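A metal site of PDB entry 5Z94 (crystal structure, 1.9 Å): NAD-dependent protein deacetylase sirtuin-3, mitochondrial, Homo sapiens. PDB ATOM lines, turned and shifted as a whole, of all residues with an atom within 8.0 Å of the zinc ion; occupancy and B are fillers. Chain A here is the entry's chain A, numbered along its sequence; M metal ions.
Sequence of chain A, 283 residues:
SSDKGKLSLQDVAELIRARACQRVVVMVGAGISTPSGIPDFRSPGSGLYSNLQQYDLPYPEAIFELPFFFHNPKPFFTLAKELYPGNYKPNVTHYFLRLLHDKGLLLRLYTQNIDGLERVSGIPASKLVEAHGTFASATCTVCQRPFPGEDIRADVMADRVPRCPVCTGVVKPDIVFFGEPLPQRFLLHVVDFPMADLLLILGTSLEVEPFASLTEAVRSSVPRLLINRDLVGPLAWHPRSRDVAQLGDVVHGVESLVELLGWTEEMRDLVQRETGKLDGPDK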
ATOM      1  N   THR A 139      -7.065  12.429   3.168  1.00  0.00           N
ATOM      2  CA  THR A 139      -8.472  12.407   2.749  1.00  0.00           C
ATOM      3  C   THR A 139      -8.876  10.990   2.399  1.00  0.00           C
ATOM      4  O   THR A 139      -8.168  10.298   1.654  1.00  0.00           O
ATOM      5  CB  THR A 139      -8.691  13.332   1.539  1.00  0.00           C
ATOM      6  OG1 THR A 139      -8.262  14.658   1.875  1.00  0.00           O
ATOM      7  CG2 THR A 139     -10.172  13.388   1.151  1.00  0.00           C
ATOM      8  N   CYS A 140     -10.025  10.538   2.910  1.00  0.00           N
ATOM      9  CA  CYS A 140     -10.516   9.222   2.488  1.00  0.00           C
ATOM     10  C   CYS A 140     -10.865   9.241   1.004  1.00  0.00           C
ATOM     11  O   CYS A 140     -11.627  10.097   0.547  1.00  0.00           O
ATOM     12  CB  CYS A 140     -11.745   8.798   3.295  1.00  0.00           C
ATOM     13  SG  CYS A 140     -12.403   7.202   2.745  1.00  0.00           S
ATOM     14  N   THR A 141     -10.320   8.286   0.265  1.00  0.00           N
ATOM     15  CA  THR A 141     -10.563   8.236  -1.175  1.00  0.00           C
ATOM     16  C   THR A 141     -12.011   7.926  -1.519  1.00  0.00           C
ATOM     17  O   THR A 141     -12.420   8.152  -2.668  1.00  0.00           O
ATOM     18  CB  THR A 141      -9.658   7.186  -1.832  1.00  0.00           C
ATOM     19  OG1 THR A 141      -9.875   5.921  -1.189  1.00  0.00           O
ATOM     20  CG2 THR A 141      -8.194   7.607  -1.696  1.00  0.00           C
ATOM     21  N   VAL A 142     -12.791   7.397  -0.574  1.00  0.00           N
ATOM     22  CA  VAL A 142     -14.178   7.027  -0.830  1.00  0.00           C
ATOM     23  C   VAL A 142     -15.132   8.089  -0.294  1.00  0.00           C
ATOM     24  O   VAL A 142     -15.885   8.698  -1.059  1.00  0.00           O
ATOM     25  CB  VAL A 142     -14.500   5.636  -0.244  1.00  0.00           C
ATOM     26  CG1 VAL A 142     -15.998   5.324  -0.426  1.00  0.00           C
ATOM     27  CG2 VAL A 142     -13.637   4.547  -0.918  1.00  0.00           C
ATOM     28  N   CYS A 143     -15.115   8.349   1.019  1.00  0.00           N
ATOM     29  CA  CYS A 143     -16.149   9.230   1.564  1.00  0.00           C
ATOM     30  C   CYS A 143     -15.705  10.694   1.671  1.00  0.00           C
ATOM     31  O   CYS A 143     -16.522  11.545   2.057  1.00  0.00           O
ATOM     32  CB  CYS A 143     -16.609   8.739   2.934  1.00  0.00           C
ATOM     33  SG  CYS A 143     -15.414   8.943   4.269  1.00  0.00           S
ATOM     34  N   GLN A 144     -14.456  10.996   1.354  1.00  0.00           N
ATOM     35  CA  GLN A 144     -13.865  12.335   1.348  1.00  0.00           C
ATOM     36  C   GLN A 144     -13.726  12.963   2.737  1.00  0.00           C
ATOM     37  O   GLN A 144     -13.463  14.165   2.835  1.00  0.00           O
ATOM     38  CB  GLN A 144     -14.655  13.289   0.436  1.00  0.00           C
ATOM     39  CG  GLN A 144     -14.930  12.702  -0.956  1.00  0.00           C
ATOM     40  CD  GLN A 144     -13.676  12.263  -1.667  1.00  0.00           C
ATOM     41  OE1 GLN A 144     -12.643  12.941  -1.617  1.00  0.00           O
ATOM     42  NE2 GLN A 144     -13.750  11.123  -2.347  1.00  0.00           N
ATOM     43  N   ARG A 145     -13.833  12.181   3.801  1.00  0.00           N
ATOM     44  CA  ARG A 145     -13.543  12.702   5.127  1.00  0.00           C
ATOM     45  C   ARG A 145     -12.094  13.153   5.246  1.00  0.00           C
ATOM     46  O   ARG A 145     -11.180  12.408   4.848  1.00  0.00           O
ATOM     47  CB  ARG A 145     -13.817  11.643   6.189  1.00  0.00           C
ATOM     48  CG  ARG A 145     -15.224  11.697   6.729  1.00  0.00           C
ATOM     49  CD  ARG A 145     -15.432  10.689   7.832  1.00  0.00           C
ATOM     50  NE  ARG A 145     -16.799  10.728   8.340  1.00  0.00           N
ATOM     51  CZ  ARG A 145     -17.840  10.185   7.713  1.00  0.00           C
ATOM     52  NH1 ARG A 145     -17.671   9.560   6.554  1.00  0.00           N
ATOM     53  NH2 ARG A 145     -19.051  10.267   8.245  1.00  0.00           N
ATOM     54  N   PRO A 146     -11.834  14.320   5.806  1.00  0.00           N
ATOM     55  CA  PRO A 146     -10.447  14.754   6.050  1.00  0.00           C
ATOM     56  C   PRO A 146      -9.940  14.219   7.378  1.00  0.00           C
ATOM     57  O   PRO A 146     -10.694  14.017   8.325  1.00  0.00           O
ATOM     58  CB  PRO A 146     -10.565  16.280   6.095  1.00  0.00           C
ATOM     59  CG  PRO A 146     -11.937  16.506   6.703  1.00  0.00           C
ATOM     60  CD  PRO A 146     -12.814  15.349   6.225  1.00  0.00           C
ATOM     61  N   PHE A 147      -8.624  14.019   7.445  1.00  0.00           N
ATOM     62  CA  PHE A 147      -7.958  13.588   8.670  1.00  0.00           C
ATOM     63  C   PHE A 147      -6.641  14.343   8.850  1.00  0.00           C
ATOM     64  O   PHE A 147      -5.959  14.638   7.858  1.00  0.00           O
ATOM     65  CB  PHE A 147      -7.661  12.083   8.663  1.00  0.00           C
ATOM     66  CG  PHE A 147      -8.881  11.227   8.468  1.00  0.00           C
ATOM     67  CD1 PHE A 147      -9.228  10.776   7.208  1.00  0.00           C
ATOM     68  CD2 PHE A 147      -9.672  10.862   9.557  1.00  0.00           C
ATOM     69  CE1 PHE A 147     -10.353   9.972   7.024  1.00  0.00           C
ATOM     70  CE2 PHE A 147     -10.807  10.060   9.387  1.00  0.00           C
ATOM     71  CZ  PHE A 147     -11.142   9.621   8.113  1.00  0.00           C
ATOM     72  N   ARG A 163      -6.743   2.847   6.500  1.00  0.00           N
ATOM     73  CA  ARG A 163      -8.124   2.762   6.054  1.00  0.00           C
ATOM     74  C   ARG A 163      -8.998   3.707   6.873  1.00  0.00           C
ATOM     75  O   ARG A 163      -8.689   4.039   8.022  1.00  0.00           O
ATOM     76  CB  ARG A 163      -8.680   1.335   6.200  1.00  0.00           C
ATOM     77  CG  ARG A 163      -7.698   0.202   5.826  1.00  0.00           C
ATOM     78  CD  ARG A 163      -7.373   0.102   4.340  1.00  0.00           C
ATOM     79  NE  ARG A 163      -8.562   0.050   3.490  1.00  0.00           N
ATOM     80  CZ  ARG A 163      -8.628  -0.536   2.296  1.00  0.00           C
ATOM     81  NH1 ARG A 163      -9.756  -0.476   1.612  1.00  0.00           N
ATOM     82  NH2 ARG A 163      -7.582  -1.181   1.781  1.00  0.00           N
ATOM     83  N   CYS A 164     -10.112   4.094   6.277  1.00  0.00           N
ATOM     84  CA  CYS A 164     -11.057   5.012   6.899  1.00  0.00           C
ATOM     85  C   CYS A 164     -11.800   4.314   8.037  1.00  0.00           C
ATOM     86  O   CYS A 164     -12.335   3.222   7.841  1.00  0.00           O
ATOM     87  CB  CYS A 164     -12.045   5.517   5.853  1.00  0.00           C
ATOM     88  SG  CYS A 164     -13.271   6.720   6.477  1.00  0.00           S
ATOM     89  N   PRO A 165     -11.882   4.922   9.223  1.00  0.00           N
ATOM     90  CA  PRO A 165     -12.626   4.292  10.318  1.00  0.00           C
ATOM     91  C   PRO A 165     -14.134   4.332  10.127  1.00  0.00           C
ATOM     92  O   PRO A 165     -14.848   3.649  10.880  1.00  0.00           O
ATOM     93  CB  PRO A 165     -12.216   5.112  11.556  1.00  0.00           C
ATOM     94  CG  PRO A 165     -11.867   6.465  11.005  1.00  0.00           C
ATOM     95  CD  PRO A 165     -11.246   6.195   9.634  1.00  0.00           C
ATOM     96  N   VAL A 166     -14.647   5.082   9.158  1.00  0.00           N
ATOM     97  CA  VAL A 166     -16.072   5.132   8.889  1.00  0.00           C
ATOM     98  C   VAL A 166     -16.467   4.210   7.734  1.00  0.00           C
ATOM     99  O   VAL A 166     -17.429   3.455   7.844  1.00  0.00           O
ATOM    100  CB  VAL A 166     -16.528   6.584   8.642  1.00  0.00           C
ATOM    101  CG1 VAL A 166     -18.021   6.624   8.300  1.00  0.00           C
ATOM    102  CG2 VAL A 166     -16.235   7.448   9.862  1.00  0.00           C
ATOM    103  N   CYS A 167     -15.741   4.252   6.612  1.00  0.00           N
ATOM    104  CA  CYS A 167     -16.184   3.485   5.435  1.00  0.00           C
ATOM    105  C   CYS A 167     -15.200   2.436   4.943  1.00  0.00           C
ATOM    106  O   CYS A 167     -15.537   1.701   4.004  1.00  0.00           O
ATOM    107  CB  CYS A 167     -16.531   4.433   4.284  1.00  0.00           C
ATOM    108  SG  CYS A 167     -15.099   5.123   3.407  1.00  0.00           S
ATOM    109  N   THR A 168     -14.030   2.315   5.575  1.00  0.00           N
ATOM    110  CA  THR A 168     -12.905   1.432   5.263  1.00  0.00           C
ATOM    111  C   THR A 168     -12.196   1.777   3.959  1.00  0.00           C
ATOM    112  O   THR A 168     -11.327   1.025   3.564  1.00  0.00           O
ATOM    113  CB  THR A 168     -13.273  -0.074   5.208  1.00  0.00           C
ATOM    114  OG1 THR A 168     -14.017  -0.397   4.023  1.00  0.00           O
ATOM    115  CG2 THR A 168     -14.050  -0.480   6.441  1.00  0.00           C
ATOM    116  N   GLY A 169     -12.516   2.890   3.306  1.00  0.00           N
ATOM    117  CA  GLY A 169     -11.769   3.290   2.124  1.00  0.00           C
ATOM    118  C   GLY A 169     -10.304   3.568   2.443  1.00  0.00           C
ATOM    119  O   GLY A 169      -9.937   3.856   3.587  1.00  0.00           O
ATOM    120  N   VAL A 170      -9.450   3.448   1.414  1.00  0.00           N
ATOM    121  CA  VAL A 170      -8.044   3.832   1.601  1.00  0.00           C
ATOM    122  C   VAL A 170      -7.966   5.327   1.891  1.00  0.00           C
ATOM    123  O   VAL A 170      -8.631   6.125   1.239  1.00  0.00           O
ATOM    124  CB  VAL A 170      -7.192   3.502   0.360  1.00  0.00           C
ATOM    125  CG1 VAL A 170      -5.771   4.138   0.502  1.00  0.00           C
ATOM    126  CG2 VAL A 170      -7.095   1.971   0.122  1.00  0.00           C
ATOM    127  N   VAL A 171      -7.189   5.703   2.907  1.00  0.00           N
ATOM    128  CA  VAL A 171      -7.006   7.110   3.273  1.00  0.00           C
ATOM    129  C   VAL A 171      -5.703   7.580   2.641  1.00  0.00           C
ATOM    130  O   VAL A 171      -4.638   7.017   2.922  1.00  0.00           O
ATOM    131  CB  VAL A 171      -7.000   7.301   4.791  1.00  0.00           C
ATOM    132  CG1 VAL A 171      -6.650   8.749   5.168  1.00  0.00           C
ATOM    133  CG2 VAL A 171      -8.383   6.896   5.372  1.00  0.00           C
HETATM  134 ZN    ZN M   1     -14.173   6.998   4.346  1.00  0.00          ZN
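The zinc ion is bound by SG of Cys 167 (2.3 Å), SG of Cys 143 (2.3 Å), SG of Cys 164 (2.3 Å) and SG of Cys 140 (2.4 Å).
The side-chain sulfur of Cys 167 sits close to the backbone NH of Gly 169 (3.4 Å).
The side-chain sulfur of Cys 143 sits close to the guanidinium group of Arg 145.
The backbone NH (N) of Cys 164 lies within hydrogen-bond range of the backbone carbonyl oxygen (O) of Gly 169, 2.7 Å away.
SG of Cys 164 sits close to N of Val 166.
SG of Cys 140 lies close to N of Val 142 (3.3 Å).
N of Cys 140 sits at hydrogen-bond distance from O of Arg 145, 2.9 Å away.
Four residues have an atom within 4 Å of the zinc ion: Cys 140, Cys 143, Cys 164 and Cys 167.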
